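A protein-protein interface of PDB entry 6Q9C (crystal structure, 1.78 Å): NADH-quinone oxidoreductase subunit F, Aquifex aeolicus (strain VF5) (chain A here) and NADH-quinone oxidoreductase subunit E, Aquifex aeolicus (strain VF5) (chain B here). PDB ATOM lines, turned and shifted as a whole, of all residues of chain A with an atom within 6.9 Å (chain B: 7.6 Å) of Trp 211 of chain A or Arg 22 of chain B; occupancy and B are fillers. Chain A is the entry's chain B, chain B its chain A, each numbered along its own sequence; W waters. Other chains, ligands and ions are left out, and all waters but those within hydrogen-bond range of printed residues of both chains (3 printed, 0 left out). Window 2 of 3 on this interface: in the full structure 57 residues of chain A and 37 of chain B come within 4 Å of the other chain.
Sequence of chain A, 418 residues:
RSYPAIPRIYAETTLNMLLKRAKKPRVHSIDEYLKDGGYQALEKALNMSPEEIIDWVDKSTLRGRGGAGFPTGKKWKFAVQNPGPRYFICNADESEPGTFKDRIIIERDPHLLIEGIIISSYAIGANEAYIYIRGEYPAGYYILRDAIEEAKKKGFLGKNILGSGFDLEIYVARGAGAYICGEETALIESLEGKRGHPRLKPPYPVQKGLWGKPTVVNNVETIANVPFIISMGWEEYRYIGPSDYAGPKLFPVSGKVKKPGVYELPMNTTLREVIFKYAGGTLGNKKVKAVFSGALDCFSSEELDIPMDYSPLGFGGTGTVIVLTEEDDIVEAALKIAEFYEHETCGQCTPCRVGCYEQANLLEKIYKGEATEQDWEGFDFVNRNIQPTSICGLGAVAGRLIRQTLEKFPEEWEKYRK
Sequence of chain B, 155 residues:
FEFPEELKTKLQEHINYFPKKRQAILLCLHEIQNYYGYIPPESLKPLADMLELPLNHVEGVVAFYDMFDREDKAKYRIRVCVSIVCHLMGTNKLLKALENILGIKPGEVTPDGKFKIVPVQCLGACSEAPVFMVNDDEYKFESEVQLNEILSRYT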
ATOM      1  N   TYR A  87     -21.213 -23.784 -36.310  1.00  0.00           N
ATOM      2  CA  TYR A  87     -19.769 -23.636 -36.597  1.00  0.00           C
ATOM      3  C   TYR A  87     -19.442 -24.409 -37.866  1.00  0.00           C
ATOM      4  O   TYR A  87     -20.063 -25.461 -38.133  1.00  0.00           O
ATOM      5  CB  TYR A  87     -18.936 -24.104 -35.407  1.00  0.00           C
ATOM      6  CG  TYR A  87     -19.207 -23.335 -34.142  1.00  0.00           C
ATOM      7  CD1 TYR A  87     -18.836 -22.007 -34.024  1.00  0.00           C
ATOM      8  CD2 TYR A  87     -19.842 -23.930 -33.064  1.00  0.00           C
ATOM      9  CE1 TYR A  87     -19.081 -21.291 -32.862  1.00  0.00           C
ATOM     10  CE2 TYR A  87     -20.098 -23.226 -31.900  1.00  0.00           C
ATOM     11  CZ  TYR A  87     -19.720 -21.900 -31.799  1.00  0.00           C
ATOM     12  OH  TYR A  87     -19.973 -21.205 -30.652  1.00  0.00           O
ATOM     13  N   GLU A 128     -18.434 -18.167 -37.359  1.00  0.00           N
ATOM     14  CA  GLU A 128     -17.131 -18.597 -36.799  1.00  0.00           C
ATOM     15  C   GLU A 128     -16.738 -19.902 -37.498  1.00  0.00           C
ATOM     16  O   GLU A 128     -17.515 -20.874 -37.425  1.00  0.00           O
ATOM     17  CB  GLU A 128     -17.285 -18.710 -35.281  1.00  0.00           C
ATOM     18  CG  GLU A 128     -16.053 -19.196 -34.540  1.00  0.00           C
ATOM     19  CD  GLU A 128     -16.205 -19.185 -33.026  1.00  0.00           C
ATOM     20  OE1 GLU A 128     -16.814 -18.237 -32.516  1.00  0.00           O
ATOM     21  OE2 GLU A 128     -15.713 -20.133 -32.359  1.00  0.00           O
ATOM     22  N   TYR A 130     -13.255 -22.611 -38.478  1.00  0.00           N
ATOM     23  CA  TYR A 130     -11.912 -23.064 -38.053  1.00  0.00           C
ATOM     24  C   TYR A 130     -11.262 -23.827 -39.199  1.00  0.00           C
ATOM     25  O   TYR A 130     -11.966 -24.532 -39.947  1.00  0.00           O
ATOM     26  CB  TYR A 130     -12.001 -23.946 -36.809  1.00  0.00           C
ATOM     27  CG  TYR A 130     -12.411 -23.203 -35.569  1.00  0.00           C
ATOM     28  CD1 TYR A 130     -13.743 -22.940 -35.297  1.00  0.00           C
ATOM     29  CD2 TYR A 130     -11.458 -22.741 -34.678  1.00  0.00           C
ATOM     30  CE1 TYR A 130     -14.117 -22.246 -34.157  1.00  0.00           C
ATOM     31  CE2 TYR A 130     -11.816 -22.064 -33.531  1.00  0.00           C
ATOM     32  CZ  TYR A 130     -13.147 -21.807 -33.272  1.00  0.00           C
ATOM     33  OH  TYR A 130     -13.477 -21.129 -32.137  1.00  0.00           O
ATOM     34  N   ILE A 188     -12.773 -31.800 -32.903  1.00  0.00           N
ATOM     35  CA  ILE A 188     -13.599 -30.862 -32.093  1.00  0.00           C
ATOM     36  C   ILE A 188     -13.079 -30.860 -30.647  1.00  0.00           C
ATOM     37  O   ILE A 188     -12.882 -29.761 -30.110  1.00  0.00           O
ATOM     38  CB  ILE A 188     -15.094 -31.209 -32.226  1.00  0.00           C
ATOM     39  CG1 ILE A 188     -15.598 -30.859 -33.630  1.00  0.00           C
ATOM     40  CG2 ILE A 188     -15.920 -30.528 -31.147  1.00  0.00           C
ATOM     41  CD1 ILE A 188     -16.903 -31.508 -34.010  1.00  0.00           C
ATOM     42  N   SER A 190     -10.065 -31.431 -29.622  1.00  0.00           N
ATOM     43  CA  SER A 190      -8.749 -30.744 -29.704  1.00  0.00           C
ATOM     44  C   SER A 190      -8.964 -29.226 -29.840  1.00  0.00           C
ATOM     45  O   SER A 190      -8.242 -28.456 -29.177  1.00  0.00           O
ATOM     46  CB  SER A 190      -7.916 -31.303 -30.834  1.00  0.00           C
ATOM     47  OG  SER A 190      -6.583 -30.825 -30.759  1.00  0.00           O
ATOM     48  N   LEU A 191      -9.947 -28.811 -30.639  1.00  0.00           N
ATOM     49  CA  LEU A 191     -10.324 -27.380 -30.807  1.00  0.00           C
ATOM     50  C   LEU A 191     -10.821 -26.804 -29.474  1.00  0.00           C
ATOM     51  O   LEU A 191     -10.689 -25.589 -29.286  1.00  0.00           O
ATOM     52  CB  LEU A 191     -11.414 -27.250 -31.872  1.00  0.00           C
ATOM     53  CG  LEU A 191     -10.948 -27.105 -33.312  1.00  0.00           C
ATOM     54  CD1 LEU A 191     -12.152 -26.966 -34.226  1.00  0.00           C
ATOM     55  CD2 LEU A 191     -10.003 -25.922 -33.482  1.00  0.00           C
ATOM     56  N   GLU A 192     -11.388 -27.638 -28.599  1.00  0.00           N
ATOM     57  CA  GLU A 192     -11.900 -27.238 -27.263  1.00  0.00           C
ATOM     58  C   GLU A 192     -10.750 -27.246 -26.238  1.00  0.00           C
ATOM     59  O   GLU A 192     -11.012 -26.977 -25.048  1.00  0.00           O
ATOM     60  CB  GLU A 192     -13.056 -28.154 -26.851  1.00  0.00           C
ATOM     61  CG  GLU A 192     -14.313 -27.982 -27.695  1.00  0.00           C
ATOM     62  CD  GLU A 192     -15.515 -28.812 -27.254  1.00  0.00           C
ATOM     63  OE1 GLU A 192     -16.601 -28.658 -27.849  1.00  0.00           O
ATOM     64  OE2 GLU A 192     -15.368 -29.611 -26.311  1.00  0.00           O
ATOM     65  N   GLY A 193      -9.527 -27.561 -26.670  1.00  0.00           N
ATOM     66  CA  GLY A 193      -8.314 -27.497 -25.832  1.00  0.00           C
ATOM     67  C   GLY A 193      -8.100 -28.765 -25.029  1.00  0.00           C
ATOM     68  O   GLY A 193      -7.421 -28.701 -23.980  1.00  0.00           O
ATOM     69  N   LYS A 194      -8.635 -29.892 -25.504  1.00  0.00           N
ATOM     70  CA  LYS A 194      -8.544 -31.192 -24.783  1.00  0.00           C
ATOM     71  C   LYS A 194      -7.736 -32.193 -25.609  1.00  0.00           C
ATOM     72  O   LYS A 194      -7.345 -31.868 -26.746  1.00  0.00           O
ATOM     73  CB  LYS A 194      -9.941 -31.737 -24.481  1.00  0.00           C
ATOM     74  CG  LYS A 194     -10.708 -30.961 -23.422  1.00  0.00           C
ATOM     75  CD  LYS A 194     -12.164 -31.347 -23.332  1.00  0.00           C
ATOM     76  CE  LYS A 194     -12.964 -30.821 -24.502  1.00  0.00           C
ATOM     77  NZ  LYS A 194     -14.417 -31.035 -24.312  1.00  0.00           N
ATOM     78  N   ARG A 199     -15.770 -38.902 -29.784  1.00  0.00           N
ATOM     79  CA  ARG A 199     -17.050 -38.983 -29.038  1.00  0.00           C
ATOM     80  C   ARG A 199     -17.911 -40.094 -29.639  1.00  0.00           C
ATOM     81  O   ARG A 199     -17.859 -40.289 -30.874  1.00  0.00           O
ATOM     82  CB  ARG A 199     -17.819 -37.665 -29.141  1.00  0.00           C
ATOM     83  CG  ARG A 199     -17.059 -36.448 -28.642  1.00  0.00           C
ATOM     84  CD  ARG A 199     -17.854 -35.212 -29.001  1.00  0.00           C
ATOM     85  NE  ARG A 199     -17.271 -33.987 -28.480  1.00  0.00           N
ATOM     86  CZ  ARG A 199     -17.765 -32.770 -28.683  1.00  0.00           C
ATOM     87  NH1 ARG A 199     -17.153 -31.720 -28.161  1.00  0.00           N
ATOM     88  NH2 ARG A 199     -18.867 -32.608 -29.400  1.00  0.00           N
ATOM     89  N   LYS A 208     -24.658 -31.991 -32.610  1.00  0.00           N
ATOM     90  CA  LYS A 208     -23.908 -31.555 -31.396  1.00  0.00           C
ATOM     91  C   LYS A 208     -22.404 -31.659 -31.668  1.00  0.00           C
ATOM     92  O   LYS A 208     -21.891 -32.791 -31.734  1.00  0.00           O
ATOM     93  CB  LYS A 208     -24.296 -32.397 -30.174  1.00  0.00           C
ATOM     94  CG  LYS A 208     -25.619 -32.019 -29.523  1.00  0.00           C
ATOM     95  CD  LYS A 208     -25.772 -32.521 -28.090  1.00  0.00           C
ATOM     96  CE  LYS A 208     -26.638 -31.620 -27.232  1.00  0.00           C
ATOM     97  NZ  LYS A 208     -26.034 -30.273 -27.062  1.00  0.00           N
ATOM     98  N   GLY A 209     -21.738 -30.514 -31.835  1.00  0.00           N
ATOM     99  CA  GLY A 209     -20.310 -30.435 -32.198  1.00  0.00           C
ATOM    100  C   GLY A 209     -19.526 -29.557 -31.240  1.00  0.00           C
ATOM    101  O   GLY A 209     -19.497 -29.865 -30.032  1.00  0.00           O
ATOM    102  N   LEU A 210     -18.902 -28.508 -31.769  1.00  0.00           N
ATOM    103  CA  LEU A 210     -18.064 -27.549 -31.006  1.00  0.00           C
ATOM    104  C   LEU A 210     -18.952 -26.811 -30.001  1.00  0.00           C
ATOM    105  O   LEU A 210     -19.954 -26.213 -30.424  1.00  0.00           O
ATOM    106  CB  LEU A 210     -17.385 -26.594 -31.993  1.00  0.00           C
ATOM    107  CG  LEU A 210     -16.424 -25.582 -31.370  1.00  0.00           C
ATOM    108  CD1 LEU A 210     -15.192 -26.264 -30.801  1.00  0.00           C
ATOM    109  CD2 LEU A 210     -16.023 -24.527 -32.380  1.00  0.00           C
ATOM    110  N   TRP A 211     -18.607 -26.900 -28.714  1.00  0.00           N
ATOM    111  CA  TRP A 211     -19.374 -26.342 -27.573  1.00  0.00           C
ATOM    112  C   TRP A 211     -20.818 -26.872 -27.605  1.00  0.00           C
ATOM    113  O   TRP A 211     -21.725 -26.184 -27.096  1.00  0.00           O
ATOM    114  CB  TRP A 211     -19.302 -24.809 -27.587  1.00  0.00           C
ATOM    115  CG  TRP A 211     -17.917 -24.268 -27.790  1.00  0.00           C
ATOM    116  CD1 TRP A 211     -17.516 -23.395 -28.759  1.00  0.00           C
ATOM    117  CD2 TRP A 211     -16.737 -24.566 -27.019  1.00  0.00           C
ATOM    118  NE1 TRP A 211     -16.177 -23.132 -28.648  1.00  0.00           N
ATOM    119  CE2 TRP A 211     -15.673 -23.827 -27.582  1.00  0.00           C
ATOM    120  CE3 TRP A 211     -16.474 -25.375 -25.910  1.00  0.00           C
ATOM    121  CZ2 TRP A 211     -14.375 -23.883 -27.081  1.00  0.00           C
ATOM    122  CZ3 TRP A 211     -15.190 -25.427 -25.411  1.00  0.00           C
ATOM    123  CH2 TRP A 211     -14.156 -24.694 -25.993  1.00  0.00           C
ATOM    124  N   GLY A 212     -21.021 -28.068 -28.168  1.00  0.00           N
ATOM    125  CA  GLY A 212     -22.323 -28.761 -28.213  1.00  0.00           C
ATOM    126  C   GLY A 212     -23.265 -28.177 -29.257  1.00  0.00           C
ATOM    127  O   GLY A 212     -24.448 -28.548 -29.251  1.00  0.00           O
ATOM    128  N   LYS A 213     -22.770 -27.296 -30.129  1.00  0.00           N
ATOM    129  CA  LYS A 213     -23.596 -26.580 -31.134  1.00  0.00           C
ATOM    130  C   LYS A 213     -23.497 -27.301 -32.473  1.00  0.00           C
ATOM    131  O   LYS A 213     -22.514 -27.996 -32.738  1.00  0.00           O
ATOM    132  CB  LYS A 213     -23.144 -25.122 -31.250  1.00  0.00           C
ATOM    133  CG  LYS A 213     -23.239 -24.318 -29.961  1.00  0.00           C
ATOM    134  CD  LYS A 213     -24.655 -24.147 -29.464  1.00  0.00           C
ATOM    135  CE  LYS A 213     -24.733 -23.585 -28.057  1.00  0.00           C
ATOM    136  NZ  LYS A 213     -26.116 -23.617 -27.530  1.00  0.00           N
ATOM    137  N   PRO A 214     -24.505 -27.146 -33.361  1.00  0.00           N
ATOM    138  CA  PRO A 214     -24.440 -27.719 -34.704  1.00  0.00           C
ATOM    139  C   PRO A 214     -23.141 -27.294 -35.396  1.00  0.00           C
ATOM    140  O   PRO A 214     -22.880 -26.100 -35.500  1.00  0.00           O
ATOM    141  CB  PRO A 214     -25.672 -27.151 -35.417  1.00  0.00           C
ATOM    142  CG  PRO A 214     -26.630 -26.844 -34.292  1.00  0.00           C
ATOM    143  CD  PRO A 214     -25.758 -26.410 -33.132  1.00  0.00           C
ATOM    144  N   THR A 215     -22.369 -28.285 -35.841  1.00  0.00           N
ATOM    145  CA  THR A 215     -21.024 -28.102 -36.437  1.00  0.00           C
ATOM    146  C   THR A 215     -20.925 -28.952 -37.704  1.00  0.00           C
ATOM    147  O   THR A 215     -21.224 -30.158 -37.649  1.00  0.00           O
ATOM    148  CB  THR A 215     -19.928 -28.440 -35.421  1.00  0.00           C
ATOM    149  OG1 THR A 215     -20.143 -27.638 -34.258  1.00  0.00           O
ATOM    150  CG2 THR A 215     -18.528 -28.211 -35.944  1.00  0.00           C
ATOM    151  N   ILE B  15      -3.397 -16.869 -26.727  1.00  0.00           N
ATOM    152  CA  ILE B  15      -4.528 -16.960 -25.757  1.00  0.00           C
ATOM    153  C   ILE B  15      -5.624 -15.960 -26.161  1.00  0.00           C
ATOM    154  O   ILE B  15      -6.814 -16.287 -25.972  1.00  0.00           O
ATOM    155  CB  ILE B  15      -4.011 -16.778 -24.312  1.00  0.00           C
ATOM    156  CG1 ILE B  15      -3.191 -17.997 -23.877  1.00  0.00           C
ATOM    157  CG2 ILE B  15      -5.149 -16.493 -23.345  1.00  0.00           C
ATOM    158  CD1 ILE B  15      -2.382 -17.792 -22.616  1.00  0.00           C
ATOM    159  N   PHE B  18      -8.068 -16.943 -30.132  1.00  0.00           N
ATOM    160  CA  PHE B  18      -9.324 -17.731 -30.172  1.00  0.00           C
ATOM    161  C   PHE B  18     -10.367 -17.073 -29.272  1.00  0.00           C
ATOM    162  O   PHE B  18     -10.025 -16.288 -28.386  1.00  0.00           O
ATOM    163  CB  PHE B  18      -9.068 -19.177 -29.748  1.00  0.00           C
ATOM    164  CG  PHE B  18      -8.154 -19.957 -30.659  1.00  0.00           C
ATOM    165  CD1 PHE B  18      -8.608 -20.441 -31.872  1.00  0.00           C
ATOM    166  CD2 PHE B  18      -6.847 -20.228 -30.287  1.00  0.00           C
ATOM    167  CE1 PHE B  18      -7.769 -21.167 -32.704  1.00  0.00           C
ATOM    168  CE2 PHE B  18      -6.007 -20.949 -31.121  1.00  0.00           C
ATOM    169  CZ  PHE B  18      -6.473 -21.424 -32.324  1.00  0.00           C
ATOM    170  N   PRO B  19     -11.674 -17.340 -29.492  1.00  0.00           N
ATOM    171  CA  PRO B  19     -12.726 -16.837 -28.606  1.00  0.00           C
ATOM    172  C   PRO B  19     -12.589 -17.294 -27.144  1.00  0.00           C
ATOM    173  O   PRO B  19     -12.963 -16.527 -26.286  1.00  0.00           O
ATOM    174  CB  PRO B  19     -14.017 -17.410 -29.213  1.00  0.00           C
ATOM    175  CG  PRO B  19     -13.666 -17.625 -30.669  1.00  0.00           C
ATOM    176  CD  PRO B  19     -12.220 -18.067 -30.647  1.00  0.00           C
ATOM    177  N   LYS B  20     -12.080 -18.511 -26.904  1.00  0.00           N
ATOM    178  CA  LYS B  20     -11.861 -19.068 -25.537  1.00  0.00           C
ATOM    179  C   LYS B  20     -10.368 -19.346 -25.330  1.00  0.00           C
ATOM    180  O   LYS B  20      -9.719 -19.890 -26.244  1.00  0.00           O
ATOM    181  CB  LYS B  20     -12.730 -20.309 -25.310  1.00  0.00           C
ATOM    182  CG  LYS B  20     -14.219 -20.077 -25.530  1.00  0.00           C
ATOM    183  CD  LYS B  20     -15.105 -21.157 -24.947  1.00  0.00           C
ATOM    184  CE  LYS B  20     -16.580 -20.901 -25.169  1.00  0.00           C
ATOM    185  NZ  LYS B  20     -17.416 -21.967 -24.566  1.00  0.00           N
ATOM    186  N   LYS B  21      -9.840 -18.920 -24.181  1.00  0.00           N
ATOM    187  CA  LYS B  21      -8.398 -18.998 -23.832  1.00  0.00           C
ATOM    188  C   LYS B  21      -7.895 -20.434 -24.009  1.00  0.00           C
ATOM    189  O   LYS B  21      -6.802 -20.609 -24.565  1.00  0.00           O
ATOM    190  CB  LYS B  21      -8.161 -18.554 -22.387  1.00  0.00           C
ATOM    191  CG  LYS B  21      -8.428 -17.085 -22.104  1.00  0.00           C
ATOM    192  CD  LYS B  21      -7.945 -16.658 -20.738  1.00  0.00           C
ATOM    193  CE  LYS B  21      -8.056 -15.165 -20.511  1.00  0.00           C
ATOM    194  NZ  LYS B  21      -9.438 -14.774 -20.148  1.00  0.00           N
ATOM    195  N   ARG B  22      -8.670 -21.422 -23.554  1.00  0.00           N
ATOM    196  CA  ARG B  22      -8.222 -22.840 -23.487  1.00  0.00           C
ATOM    197  C   ARG B  22      -7.971 -23.399 -24.893  1.00  0.00           C
ATOM    198  O   ARG B  22      -7.225 -24.387 -24.986  1.00  0.00           O
ATOM    199  CB  ARG B  22      -9.206 -23.710 -22.701  1.00  0.00           C
ATOM    200  CG  ARG B  22     -10.627 -23.770 -23.243  1.00  0.00           C
ATOM    201  CD  ARG B  22     -11.464 -24.463 -22.181  1.00  0.00           C
ATOM    202  NE  ARG B  22     -12.905 -24.486 -22.377  1.00  0.00           N
ATOM    203  CZ  ARG B  22     -13.750 -23.494 -22.089  1.00  0.00           C
ATOM    204  NH1 ARG B  22     -15.047 -23.667 -22.279  1.00  0.00           N
ATOM    205  NH2 ARG B  22     -13.311 -22.331 -21.638  1.00  0.00           N
ATOM    206  N   GLN B  23      -8.541 -22.790 -25.938  1.00  0.00           N
ATOM    207  CA  GLN B  23      -8.348 -23.223 -27.351  1.00  0.00           C
ATOM    208  C   GLN B  23      -6.892 -23.002 -27.792  1.00  0.00           C
ATOM    209  O   GLN B  23      -6.475 -23.656 -28.755  1.00  0.00           O
ATOM    210  CB  GLN B  23      -9.302 -22.485 -28.290  1.00  0.00           C
ATOM    211  CG  GLN B  23     -10.775 -22.721 -27.984  1.00  0.00           C
ATOM    212  CD  GLN B  23     -11.670 -22.146 -29.055  1.00  0.00           C
ATOM    213  OE1 GLN B  23     -12.120 -21.002 -28.972  1.00  0.00           O
ATOM    214  NE2 GLN B  23     -11.916 -22.934 -30.090  1.00  0.00           N
ATOM    215  N   ALA B  24      -6.140 -22.127 -27.115  1.00  0.00           N
ATOM    216  CA  ALA B  24      -4.754 -21.754 -27.488  1.00  0.00           C
ATOM    217  C   ALA B  24      -3.724 -22.771 -26.967  1.00  0.00           C
ATOM    218  O   ALA B  24      -2.528 -22.562 -27.225  1.00  0.00           O
ATOM    219  CB  ALA B  24      -4.451 -20.369 -26.973  1.00  0.00           C
ATOM    220  N   ILE B  25      -4.144 -23.825 -26.261  1.00  0.00           N
ATOM    221  CA  ILE B  25      -3.219 -24.715 -25.493  1.00  0.00           C
ATOM    222  C   ILE B  25      -2.126 -25.297 -26.406  1.00  0.00           C
ATOM    223  O   ILE B  25      -0.957 -25.271 -25.988  1.00  0.00           O
ATOM    224  CB  ILE B  25      -3.982 -25.806 -24.712  1.00  0.00           C
ATOM    225  CG1 ILE B  25      -3.029 -26.587 -23.804  1.00  0.00           C
ATOM    226  CG2 ILE B  25      -4.772 -26.725 -25.634  1.00  0.00           C
ATOM    227  CD1 ILE B  25      -3.727 -27.409 -22.752  1.00  0.00           C
ATOM    228  N   LEU B  26      -2.466 -25.799 -27.597  1.00  0.00           N
ATOM    229  CA  LEU B  26      -1.486 -26.452 -28.508  1.00  0.00           C
ATOM    230  C   LEU B  26      -0.545 -25.399 -29.111  1.00  0.00           C
ATOM    231  O   LEU B  26       0.662 -25.675 -29.198  1.00  0.00           O
ATOM    232  CB  LEU B  26      -2.227 -27.241 -29.592  1.00  0.00           C
ATOM    233  CG  LEU B  26      -3.091 -28.402 -29.093  1.00  0.00           C
ATOM    234  CD1 LEU B  26      -3.573 -29.259 -30.254  1.00  0.00           C
ATOM    235  CD2 LEU B  26      -2.339 -29.259 -28.090  1.00  0.00           C
ATOM    236  N   MET B  50      -2.246 -19.209 -17.078  1.00  0.00           N
ATOM    237  CA  MET B  50      -2.518 -18.285 -18.216  1.00  0.00           C
ATOM    238  C   MET B  50      -3.738 -18.766 -19.018  1.00  0.00           C
ATOM    239  O   MET B  50      -4.474 -17.898 -19.530  1.00  0.00           O
ATOM    240  CB  MET B  50      -1.310 -18.187 -19.153  1.00  0.00           C
ATOM    241  CG  MET B  50      -0.109 -17.506 -18.535  1.00  0.00           C
ATOM    242  SD  MET B  50       1.253 -17.333 -19.712  1.00  0.00           S
ATOM    243  CE  MET B  50       0.677 -15.951 -20.696  1.00  0.00           C
ATOM    244  N   LEU B  51      -3.938 -20.087 -19.135  1.00  0.00           N
ATOM    245  CA  LEU B  51      -5.062 -20.708 -19.892  1.00  0.00           C
ATOM    246  C   LEU B  51      -6.301 -20.861 -18.998  1.00  0.00           C
ATOM    247  O   LEU B  51      -7.372 -21.206 -19.542  1.00  0.00           O
ATOM    248  CB  LEU B  51      -4.618 -22.078 -20.428  1.00  0.00           C
ATOM    249  CG  LEU B  51      -3.515 -22.060 -21.485  1.00  0.00           C
ATOM    250  CD1 LEU B  51      -2.964 -23.457 -21.716  1.00  0.00           C
ATOM    251  CD2 LEU B  51      -4.018 -21.464 -22.790  1.00  0.00           C
ATOM    252  N   GLU B  52      -6.162 -20.634 -17.687  1.00  0.00           N
ATOM    253  CA  GLU B  52      -7.233 -20.816 -16.668  1.00  0.00           C
ATOM    254  C   GLU B  52      -7.728 -22.267 -16.732  1.00  0.00           C
ATOM    255  O   GLU B  52      -8.957 -22.484 -16.738  1.00  0.00           O
ATOM    256  CB  GLU B  52      -8.365 -19.803 -16.877  1.00  0.00           C
ATOM    257  CG  GLU B  52      -7.919 -18.361 -16.714  1.00  0.00           C
ATOM    258  CD  GLU B  52      -8.984 -17.314 -17.003  1.00  0.00           C
ATOM    259  OE1 GLU B  52      -8.683 -16.118 -16.831  1.00  0.00           O
ATOM    260  OE2 GLU B  52     -10.105 -17.692 -17.407  1.00  0.00           O
ATOM    261  N   LEU B  53      -6.788 -23.214 -16.796  1.00  0.00           N
ATOM    262  CA  LEU B  53      -7.045 -24.678 -16.783  1.00  0.00           C
ATOM    263  C   LEU B  53      -6.337 -25.281 -15.576  1.00  0.00           C
ATOM    264  O   LEU B  53      -5.347 -24.727 -15.106  1.00  0.00           O
ATOM    265  CB  LEU B  53      -6.523 -25.300 -18.082  1.00  0.00           C
ATOM    266  CG  LEU B  53      -7.358 -25.037 -19.334  1.00  0.00           C
ATOM    267  CD1 LEU B  53      -6.643 -25.557 -20.573  1.00  0.00           C
ATOM    268  CD2 LEU B  53      -8.743 -25.655 -19.211  1.00  0.00           C
ATOM    269  N   HIS B  57      -4.851 -31.121 -16.401  1.00  0.00           N
ATOM    270  CA  HIS B  57      -5.394 -30.983 -17.781  1.00  0.00           C
ATOM    271  C   HIS B  57      -4.239 -30.718 -18.750  1.00  0.00           C
ATOM    272  O   HIS B  57      -4.119 -31.449 -19.749  1.00  0.00           O
ATOM    273  CB  HIS B  57      -6.443 -29.863 -17.837  1.00  0.00           C
ATOM    274  CG  HIS B  57      -7.057 -29.655 -19.181  1.00  0.00           C
ATOM    275  ND1 HIS B  57      -8.422 -29.534 -19.352  1.00  0.00           N
ATOM    276  CD2 HIS B  57      -6.513 -29.542 -20.412  1.00  0.00           C
ATOM    277  CE1 HIS B  57      -8.687 -29.347 -20.629  1.00  0.00           C
ATOM    278  NE2 HIS B  57      -7.536 -29.350 -21.299  1.00  0.00           N
ATOM    279  N   VAL B  61      -2.562 -33.178 -21.721  1.00  0.00           N
ATOM    280  CA  VAL B  61      -2.467 -32.703 -23.130  1.00  0.00           C
ATOM    281  C   VAL B  61      -1.014 -32.871 -23.602  1.00  0.00           C
ATOM    282  O   VAL B  61      -0.833 -33.420 -24.704  1.00  0.00           O
ATOM    283  CB  VAL B  61      -3.010 -31.267 -23.284  1.00  0.00           C
ATOM    284  CG1 VAL B  61      -2.501 -30.583 -24.546  1.00  0.00           C
ATOM    285  CG2 VAL B  61      -4.532 -31.253 -23.254  1.00  0.00           C
HETATM  286  O   HOH W   1     -14.662 -20.698 -29.652  1.00  0.00           O
HETATM  287  O   HOH W   2     -12.803 -27.316 -23.068  1.00  0.00           O
HETATM  288  O   HOH W   3      -6.882 -26.531 -30.570  1.00  0.00           O
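The side-chain amide nitrogen (NE2) of Gln 23 of chain B sits at hydrogen-bond distance from the side-chain hydroxyl (OH) of Tyr 130 of chain A (3.1 Å).
The backbone carbonyl oxygen (O) of Leu 191 of chain A is in hydrogen-bond range of the side-chain amide nitrogen (NE2) of Gln 23 of chain B, at 3.0 Å.
The backbone carbonyl oxygen (O) of Gly 193 of chain A lies within hydrogen-bond range of a ring nitrogen (NE2) of His 57 of chain B, at 2.8 Å.
OE1 of Gln 23 of chain B lies within hydrogen-bond range of N of Lys 20 of chain B, 3.2 Å away.
OE2 of Glu 128 of chain A lies within hydrogen-bond range of OH of Tyr 130 of chain A (2.5 Å).
The side-chain carboxylate of Glu 192 of chain A is in salt-bridge range of the side-chain amino group of Lys 194 of chain A (2.6 Å).
The side-chain carboxylate (OE1) of Glu 192 of chain A lies within salt-bridge range of the guanidinium group (NH1) of Arg 199 of chain A, 3.1 Å away.
N of Trp 211 of chain A is in hydrogen-bond range of OE1 of Glu 192 of chain A, 2.8 Å away.
Among the printed residues, pairs that only touch across the chains: Gly 193 of chain A with Arg 22 of chain B, Ser 190 of chain A with Leu 26 of chain B, Trp 211 of chain A with Lys 20 of chain B, Trp 211 of chain A with Arg 22 of chain B, Tyr 130 of chain A with Pro 19 of chain B, Gly 193 of chain A with Ile 25 of chain B, Glu 128 of chain A with Pro 19 of chain B, Glu 192 of chain A with Arg 22 of chain B, Trp 211 of chain A with Gln 23 of chain B, Lys 194 of chain A with His 57 of chain B, Gly 193 of chain A with Val 61 of chain B and Tyr 130 of chain A with Phe 18 of chain B.
Trp 211 of chain A touches three residues of chain B.
Printed residues of chain A within 4 Å of His 57 of chain B: Gly 193 and Lys 194.
Printed residues of chain A within 4 Å of Phe 18 of chain B: Tyr 130 (3.96 Å).
Ile 188 of chain A touches none of the printed residues of chain B.
Tyr 87 of chain A touches none of the printed residues of chain B.
The nearest printed residue of chain A that does not touch Lys 20 of chain B is Tyr 130 of chain A (6.0 Å).
Of the 18 printed residues of chain A, 8 touch a printed residue of chain B.
Hydrophobic or aromatic side chains of chain A within 4 Å of the printed part of chain B: Tyr 130 and Trp 211.
Along chain A the printed residues that touch a printed residue of chain B span positions 128 to 211.
Among the printed residues, 15 pairs touch across the chains.
Among the printed residues, no Asp or Glu carboxylate lies within 4 Å of a Lys or Arg side-chain nitrogen of the other chain.
Water W1 lies within hydrogen-bond range of the side-chain amide oxygen of Gln 23 of chain B, the side-chain hydroxyl of Tyr 130 of chain A, the side-chain carboxylate of Glu 128 of chain A and the indole nitrogen of Trp 211 of chain A.
Water W2 lies within hydrogen-bond range of O of Glu 192 of chain A (2.7 Å) and NE of Arg 22 of chain B (2.9 Å).
Water W3 lies within hydrogen-bond range of the backbone carbonyl oxygen of Ser 190 of chain A (2.7 Å) and the backbone carbonyl oxygen of Gln 23 of chain B (3.4 Å).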
